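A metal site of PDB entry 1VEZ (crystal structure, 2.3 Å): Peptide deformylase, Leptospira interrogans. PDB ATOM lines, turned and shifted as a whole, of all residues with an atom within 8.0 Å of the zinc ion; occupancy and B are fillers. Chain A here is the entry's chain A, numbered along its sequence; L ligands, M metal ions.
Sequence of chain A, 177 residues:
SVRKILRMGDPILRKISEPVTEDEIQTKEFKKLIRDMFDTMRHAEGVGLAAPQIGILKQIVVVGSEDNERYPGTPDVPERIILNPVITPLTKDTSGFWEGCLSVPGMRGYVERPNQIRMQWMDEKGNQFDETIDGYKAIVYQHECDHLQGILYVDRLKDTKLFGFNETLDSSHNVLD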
ATOM      1  N   ILE A   5      38.094 -30.439 -14.695  1.00  0.00           N
ATOM      2  CA  ILE A   5      36.808 -30.441 -13.998  1.00  0.00           C
ATOM      3  C   ILE A   5      36.721 -31.699 -13.131  1.00  0.00           C
ATOM      4  O   ILE A   5      36.967 -32.804 -13.600  1.00  0.00           O
ATOM      5  CB  ILE A   5      35.629 -30.414 -15.002  1.00  0.00           C
ATOM      6  CG1 ILE A   5      35.717 -29.140 -15.841  1.00  0.00           C
ATOM      7  CG2 ILE A   5      34.300 -30.485 -14.269  1.00  0.00           C
ATOM      8  CD1 ILE A   5      34.720 -29.086 -16.999  1.00  0.00           C
ATOM      9  N   LEU A  13      33.567 -31.670  -4.280  1.00  0.00           N
ATOM     10  CA  LEU A  13      32.254 -31.334  -4.802  1.00  0.00           C
ATOM     11  C   LEU A  13      31.137 -31.387  -3.762  1.00  0.00           C
ATOM     12  O   LEU A  13      30.035 -30.907  -4.013  1.00  0.00           O
ATOM     13  CB  LEU A  13      31.895 -32.259  -5.964  1.00  0.00           C
ATOM     14  CG  LEU A  13      32.787 -32.132  -7.207  1.00  0.00           C
ATOM     15  CD1 LEU A  13      32.369 -33.145  -8.268  1.00  0.00           C
ATOM     16  CD2 LEU A  13      32.674 -30.702  -7.735  1.00  0.00           C
ATOM     17  N   VAL A  47      26.907 -24.691 -19.733  1.00  0.00           N
ATOM     18  CA  VAL A  47      26.065 -23.517 -19.690  1.00  0.00           C
ATOM     19  C   VAL A  47      26.344 -22.773 -18.377  1.00  0.00           C
ATOM     20  O   VAL A  47      25.913 -21.634 -18.176  1.00  0.00           O
ATOM     21  CB  VAL A  47      24.566 -23.908 -19.776  1.00  0.00           C
ATOM     22  CG1 VAL A  47      24.166 -24.689 -18.538  1.00  0.00           C
ATOM     23  CG2 VAL A  47      23.711 -22.655 -19.902  1.00  0.00           C
ATOM     24  N   GLY A  48      27.065 -23.435 -17.489  1.00  0.00           N
ATOM     25  CA  GLY A  48      27.405 -22.855 -16.206  1.00  0.00           C
ATOM     26  C   GLY A  48      28.556 -23.653 -15.617  1.00  0.00           C
ATOM     27  O   GLY A  48      28.805 -24.770 -16.043  1.00  0.00           O
ATOM     28  N   LEU A  49      29.244 -23.075 -14.650  1.00  0.00           N
ATOM     29  CA  LEU A  49      30.358 -23.752 -14.003  1.00  0.00           C
ATOM     30  C   LEU A  49      30.624 -23.084 -12.654  1.00  0.00           C
ATOM     31  O   LEU A  49      30.683 -21.854 -12.565  1.00  0.00           O
ATOM     32  CB  LEU A  49      31.619 -23.651 -14.863  1.00  0.00           C
ATOM     33  CG  LEU A  49      32.842 -24.348 -14.266  1.00  0.00           C
ATOM     34  CD1 LEU A  49      32.662 -25.851 -14.389  1.00  0.00           C
ATOM     35  CD2 LEU A  49      34.102 -23.905 -15.000  1.00  0.00           C
ATOM     36  N   ALA A  50      30.771 -23.897 -11.608  1.00  0.00           N
ATOM     37  CA  ALA A  50      31.025 -23.346 -10.276  1.00  0.00           C
ATOM     38  C   ALA A  50      32.457 -23.620  -9.902  1.00  0.00           C
ATOM     39  O   ALA A  50      33.013 -24.648 -10.272  1.00  0.00           O
ATOM     40  CB  ALA A  50      30.082 -23.974  -9.268  1.00  0.00           C
ATOM     41  N   GLN A  53      33.784 -27.002  -8.903  1.00  0.00           N
ATOM     42  CA  GLN A  53      33.983 -27.945  -9.985  1.00  0.00           C
ATOM     43  C   GLN A  53      35.408 -27.954 -10.490  1.00  0.00           C
ATOM     44  O   GLN A  53      35.837 -28.922 -11.124  1.00  0.00           O
ATOM     45  CB  GLN A  53      33.038 -27.652 -11.141  1.00  0.00           C
ATOM     46  CG  GLN A  53      31.580 -27.655 -10.734  1.00  0.00           C
ATOM     47  CD  GLN A  53      30.644 -27.636 -11.937  1.00  0.00           C
ATOM     48  OE1 GLN A  53      30.455 -28.664 -12.604  1.00  0.00           O
ATOM     49  NE2 GLN A  53      30.072 -26.481 -12.215  1.00  0.00           N
ATOM     50  N   ARG A  70      25.031 -29.309 -25.818  1.00  0.00           N
ATOM     51  CA  ARG A  70      24.770 -30.319 -24.813  1.00  0.00           C
ATOM     52  C   ARG A  70      23.309 -30.276 -24.375  1.00  0.00           C
ATOM     53  O   ARG A  70      22.753 -31.295 -23.962  1.00  0.00           O
ATOM     54  CB  ARG A  70      25.701 -30.142 -23.598  1.00  0.00           C
ATOM     55  CG  ARG A  70      27.076 -30.771 -23.804  1.00  0.00           C
ATOM     56  CD  ARG A  70      28.019 -30.518 -22.625  1.00  0.00           C
ATOM     57  NE  ARG A  70      27.465 -30.958 -21.349  1.00  0.00           N
ATOM     58  CZ  ARG A  70      27.030 -30.140 -20.389  1.00  0.00           C
ATOM     59  NH1 ARG A  70      27.082 -28.827 -20.552  1.00  0.00           N
ATOM     60  NH2 ARG A  70      26.544 -30.641 -19.246  1.00  0.00           N
ATOM     61  N   TYR A  71      22.684 -29.108 -24.460  1.00  0.00           N
ATOM     62  CA  TYR A  71      21.282 -28.950 -24.087  1.00  0.00           C
ATOM     63  C   TYR A  71      20.503 -28.336 -25.250  1.00  0.00           C
ATOM     64  O   TYR A  71      20.016 -27.196 -25.170  1.00  0.00           O
ATOM     65  CB  TYR A  71      21.137 -28.089 -22.827  1.00  0.00           C
ATOM     66  CG  TYR A  71      21.825 -28.658 -21.609  1.00  0.00           C
ATOM     67  CD1 TYR A  71      23.005 -28.083 -21.123  1.00  0.00           C
ATOM     68  CD2 TYR A  71      21.327 -29.788 -20.952  1.00  0.00           C
ATOM     69  CE1 TYR A  71      23.665 -28.615 -20.014  1.00  0.00           C
ATOM     70  CE2 TYR A  71      21.978 -30.333 -19.850  1.00  0.00           C
ATOM     71  CZ  TYR A  71      23.146 -29.742 -19.387  1.00  0.00           C
ATOM     72  OH  TYR A  71      23.825 -30.279 -18.308  1.00  0.00           O
ATOM     73  N   GLU A  99      18.463 -32.639 -16.489  1.00  0.00           N
ATOM     74  CA  GLU A  99      19.739 -31.996 -16.224  1.00  0.00           C
ATOM     75  C   GLU A  99      20.981 -32.852 -16.432  1.00  0.00           C
ATOM     76  O   GLU A  99      20.949 -34.088 -16.357  1.00  0.00           O
ATOM     77  CB  GLU A  99      19.757 -31.446 -14.794  1.00  0.00           C
ATOM     78  CG  GLU A  99      18.925 -30.189 -14.595  1.00  0.00           C
ATOM     79  CD  GLU A  99      18.995 -29.675 -13.169  1.00  0.00           C
ATOM     80  OE1 GLU A  99      20.106 -29.593 -12.613  1.00  0.00           O
ATOM     81  OE2 GLU A  99      17.929 -29.350 -12.614  1.00  0.00           O
ATOM     82  N   GLY A 100      22.082 -32.164 -16.691  1.00  0.00           N
ATOM     83  CA  GLY A 100      23.368 -32.794 -16.864  1.00  0.00           C
ATOM     84  C   GLY A 100      24.303 -31.961 -16.005  1.00  0.00           C
ATOM     85  O   GLY A 100      23.889 -30.960 -15.419  1.00  0.00           O
ATOM     86  N   CYS A 101      25.553 -32.366 -15.906  1.00  0.00           N
ATOM     87  CA  CYS A 101      26.503 -31.624 -15.100  1.00  0.00           C
ATOM     88  C   CYS A 101      27.896 -31.976 -15.566  1.00  0.00           C
ATOM     89  O   CYS A 101      28.199 -33.148 -15.778  1.00  0.00           O
ATOM     90  CB  CYS A 101      26.332 -31.981 -13.626  1.00  0.00           C
ATOM     91  SG  CYS A 101      27.607 -31.268 -12.538  1.00  0.00           S
ATOM     92  N   LEU A 102      28.746 -30.973 -15.728  1.00  0.00           N
ATOM     93  CA  LEU A 102      30.101 -31.223 -16.183  1.00  0.00           C
ATOM     94  C   LEU A 102      30.845 -32.148 -15.232  1.00  0.00           C
ATOM     95  O   LEU A 102      31.822 -32.786 -15.620  1.00  0.00           O
ATOM     96  CB  LEU A 102      30.845 -29.907 -16.365  1.00  0.00           C
ATOM     97  CG  LEU A 102      30.139 -28.979 -17.368  1.00  0.00           C
ATOM     98  CD1 LEU A 102      30.896 -27.669 -17.487  1.00  0.00           C
ATOM     99  CD2 LEU A 102      30.027 -29.683 -18.704  1.00  0.00           C
ATOM    100  N   SER A 103      30.381 -32.216 -13.982  1.00  0.00           N
ATOM    101  CA  SER A 103      31.002 -33.093 -12.997  1.00  0.00           C
ATOM    102  C   SER A 103      30.410 -34.510 -12.973  1.00  0.00           C
ATOM    103  O   SER A 103      30.860 -35.376 -12.220  1.00  0.00           O
ATOM    104  CB  SER A 103      30.892 -32.468 -11.599  1.00  0.00           C
ATOM    105  OG  SER A 103      31.764 -31.359 -11.487  1.00  0.00           O
ATOM    106  N   VAL A 104      29.389 -34.740 -13.798  1.00  0.00           N
ATOM    107  CA  VAL A 104      28.743 -36.043 -13.897  1.00  0.00           C
ATOM    108  C   VAL A 104      28.651 -36.318 -15.401  1.00  0.00           C
ATOM    109  O   VAL A 104      27.561 -36.420 -15.963  1.00  0.00           O
ATOM    110  CB  VAL A 104      27.323 -36.044 -13.288  1.00  0.00           C
ATOM    111  CG1 VAL A 104      26.727 -37.441 -13.319  1.00  0.00           C
ATOM    112  CG2 VAL A 104      27.383 -35.532 -11.862  1.00  0.00           C
ATOM    113  N   ARG A 113      12.750 -28.381 -10.335  1.00  0.00           N
ATOM    114  CA  ARG A 113      13.114 -27.285  -9.452  1.00  0.00           C
ATOM    115  C   ARG A 113      12.078 -26.173  -9.586  1.00  0.00           C
ATOM    116  O   ARG A 113      11.376 -26.087 -10.605  1.00  0.00           O
ATOM    117  CB  ARG A 113      14.468 -26.701  -9.829  1.00  0.00           C
ATOM    118  CG  ARG A 113      15.615 -27.679  -9.888  1.00  0.00           C
ATOM    119  CD  ARG A 113      16.853 -26.931 -10.367  1.00  0.00           C
ATOM    120  NE  ARG A 113      18.026 -27.786 -10.543  1.00  0.00           N
ATOM    121  CZ  ARG A 113      18.900 -28.063  -9.582  1.00  0.00           C
ATOM    122  NH1 ARG A 113      18.741 -27.549  -8.365  1.00  0.00           N
ATOM    123  NH2 ARG A 113      19.943 -28.834  -9.843  1.00  0.00           N
ATOM    124  N   VAL A 140      19.338 -23.202 -14.362  1.00  0.00           N
ATOM    125  CA  VAL A 140      20.786 -23.112 -14.377  1.00  0.00           C
ATOM    126  C   VAL A 140      21.356 -22.520 -13.083  1.00  0.00           C
ATOM    127  O   VAL A 140      22.332 -23.024 -12.538  1.00  0.00           O
ATOM    128  CB  VAL A 140      21.262 -22.252 -15.562  1.00  0.00           C
ATOM    129  CG1 VAL A 140      22.774 -22.035 -15.482  1.00  0.00           C
ATOM    130  CG2 VAL A 140      20.888 -22.944 -16.883  1.00  0.00           C
ATOM    131  N   HIS A 143      21.019 -24.888 -10.172  1.00  0.00           N
ATOM    132  CA  HIS A 143      21.986 -25.940 -10.374  1.00  0.00           C
ATOM    133  C   HIS A 143      23.382 -25.474  -9.964  1.00  0.00           C
ATOM    134  O   HIS A 143      24.059 -26.139  -9.175  1.00  0.00           O
ATOM    135  CB  HIS A 143      22.007 -26.364 -11.851  1.00  0.00           C
ATOM    136  CG  HIS A 143      23.000 -27.435 -12.163  1.00  0.00           C
ATOM    137  ND1 HIS A 143      22.654 -28.730 -12.507  1.00  0.00           N
ATOM    138  CD2 HIS A 143      24.353 -27.401 -12.165  1.00  0.00           C
ATOM    139  CE1 HIS A 143      23.794 -29.414 -12.685  1.00  0.00           C
ATOM    140  NE2 HIS A 143      24.847 -28.651 -12.489  1.00  0.00           N
ATOM    141  N   GLU A 144      23.803 -24.324 -10.491  1.00  0.00           N
ATOM    142  CA  GLU A 144      25.120 -23.781 -10.176  1.00  0.00           C
ATOM    143  C   GLU A 144      25.295 -23.435  -8.709  1.00  0.00           C
ATOM    144  O   GLU A 144      26.353 -23.691  -8.135  1.00  0.00           O
ATOM    145  CB  GLU A 144      25.410 -22.543 -11.023  1.00  0.00           C
ATOM    146  CG  GLU A 144      25.386 -22.791 -12.523  1.00  0.00           C
ATOM    147  CD  GLU A 144      26.073 -24.086 -12.904  1.00  0.00           C
ATOM    148  OE1 GLU A 144      27.144 -24.392 -12.331  1.00  0.00           O
ATOM    149  OE2 GLU A 144      25.548 -24.799 -13.799  1.00  0.00           O
ATOM    150  N   CYS A 145      24.272 -22.860  -8.103  1.00  0.00           N
ATOM    151  CA  CYS A 145      24.373 -22.492  -6.700  1.00  0.00           C
ATOM    152  C   CYS A 145      24.425 -23.726  -5.822  1.00  0.00           C
ATOM    153  O   CYS A 145      25.060 -23.707  -4.761  1.00  0.00           O
ATOM    154  CB  CYS A 145      23.206 -21.590  -6.289  1.00  0.00           C
ATOM    155  SG  CYS A 145      23.287 -19.977  -7.114  1.00  0.00           S
ATOM    156  N   ASP A 146      23.768 -24.808  -6.251  1.00  0.00           N
ATOM    157  CA  ASP A 146      23.796 -26.055  -5.482  1.00  0.00           C
ATOM    158  C   ASP A 146      25.260 -26.471  -5.325  1.00  0.00           C
ATOM    159  O   ASP A 146      25.681 -26.921  -4.267  1.00  0.00           O
ATOM    160  CB  ASP A 146      23.007 -27.147  -6.212  1.00  0.00           C
ATOM    161  CG  ASP A 146      21.570 -27.257  -5.733  1.00  0.00           C
ATOM    162  OD1 ASP A 146      20.789 -28.008  -6.348  1.00  0.00           O
ATOM    163  OD2 ASP A 146      21.208 -26.589  -4.735  1.00  0.00           O
ATOM    164  N   HIS A 147      26.036 -26.308  -6.388  1.00  0.00           N
ATOM    165  CA  HIS A 147      27.451 -26.657  -6.336  1.00  0.00           C
ATOM    166  C   HIS A 147      28.180 -25.977  -5.175  1.00  0.00           C
ATOM    167  O   HIS A 147      29.093 -26.559  -4.583  1.00  0.00           O
ATOM    168  CB  HIS A 147      28.149 -26.272  -7.635  1.00  0.00           C
ATOM    169  CG  HIS A 147      28.001 -27.278  -8.726  1.00  0.00           C
ATOM    170  ND1 HIS A 147      28.427 -28.583  -8.629  1.00  0.00           N
ATOM    171  CD2 HIS A 147      27.497 -27.148  -9.972  1.00  0.00           C
ATOM    172  CE1 HIS A 147      28.193 -29.182  -9.798  1.00  0.00           C
ATOM    173  NE2 HIS A 147      27.632 -28.354 -10.643  1.00  0.00           N
ATOM    174  N   ILE A 151      26.135 -29.579  -3.369  1.00  0.00           N
ATOM    175  CA  ILE A 151      25.019 -30.347  -3.870  1.00  0.00           C
ATOM    176  C   ILE A 151      25.104 -30.577  -5.377  1.00  0.00           C
ATOM    177  O   ILE A 151      25.392 -29.659  -6.139  1.00  0.00           O
ATOM    178  CB  ILE A 151      23.700 -29.608  -3.544  1.00  0.00           C
ATOM    179  CG1 ILE A 151      23.555 -29.505  -2.031  1.00  0.00           C
ATOM    180  CG2 ILE A 151      22.524 -30.315  -4.177  1.00  0.00           C
ATOM    181  CD1 ILE A 151      22.319 -28.724  -1.583  1.00  0.00           C
ATOM    182  N   LEU A 152      24.862 -31.826  -5.794  1.00  0.00           N
ATOM    183  CA  LEU A 152      24.892 -32.205  -7.208  1.00  0.00           C
ATOM    184  C   LEU A 152      23.458 -32.569  -7.597  1.00  0.00           C
ATOM    185  O   LEU A 152      22.659 -32.937  -6.737  1.00  0.00           O
ATOM    186  CB  LEU A 152      25.810 -33.414  -7.408  1.00  0.00           C
ATOM    187  CG  LEU A 152      27.286 -33.213  -7.029  1.00  0.00           C
ATOM    188  CD1 LEU A 152      28.064 -34.487  -7.345  1.00  0.00           C
ATOM    189  CD2 LEU A 152      27.875 -32.026  -7.802  1.00  0.00           C
ATOM    190  N   TYR A 153      23.135 -32.461  -8.875  1.00  0.00           N
ATOM    191  CA  TYR A 153      21.773 -32.734  -9.305  1.00  0.00           C
ATOM    192  C   TYR A 153      21.314 -34.171  -9.025  1.00  0.00           C
ATOM    193  O   TYR A 153      20.122 -34.418  -8.934  1.00  0.00           O
ATOM    194  CB  TYR A 153      21.594 -32.400 -10.795  1.00  0.00           C
ATOM    195  CG  TYR A 153      22.047 -33.454 -11.769  1.00  0.00           C
ATOM    196  CD1 TYR A 153      21.174 -34.468 -12.176  1.00  0.00           C
ATOM    197  CD2 TYR A 153      23.339 -33.445 -12.285  1.00  0.00           C
ATOM    198  CE1 TYR A 153      21.582 -35.446 -13.103  1.00  0.00           C
ATOM    199  CE2 TYR A 153      23.757 -34.408 -13.195  1.00  0.00           C
ATOM    200  CZ  TYR A 153      22.873 -35.404 -13.604  1.00  0.00           C
ATOM    201  OH  TYR A 153      23.287 -36.319 -14.534  1.00  0.00           O
HETATM  202  C1  LIG L   1      28.346 -27.335 -14.487  1.00  0.00           C
HETATM  203  O1  LIG L   1      28.346 -28.546 -14.561  1.00  0.00           O
HETATM  204  O2  LIG L   1      27.579 -26.603 -13.716  1.00  0.00           O
HETATM  205 ZN    ZN M   1      26.945 -28.929 -12.529  1.00  0.00          ZN
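A ring nitrogen (NE2) of His 147 sits close to the side-chain amide oxygen (OE1) of Gln 53 (3.5 Å).
ND1 of His 143 sits at hydrogen-bond distance from OE1 of Glu 99.
N of Ser 103 sits close to SG of Cys 101.
The side-chain hydroxyl (OG) of Ser 103 is in hydrogen-bond range of the side-chain amide oxygen (OE1) of Gln 53.
NE2 of Gln 53 lies close to N of Ala 50 (2.7 Å).
Residues that only touch the zinc ion: Gln 53.
The nearest printed residue that does not touch the zinc ion is Leu 102 (4.2 Å).
The zinc ion is bound by a ring nitrogen (NE2) of His 147, a ring nitrogen (NE2) of His 143, the side-chain sulfur (SG) of Cys 101 and an oxygen (O1) of the ligand.
The zinc ion has four donor atoms within binding distance.
Slightly farther from the zinc ion lies an oxygen (O2) of the ligand (2.7 Å).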
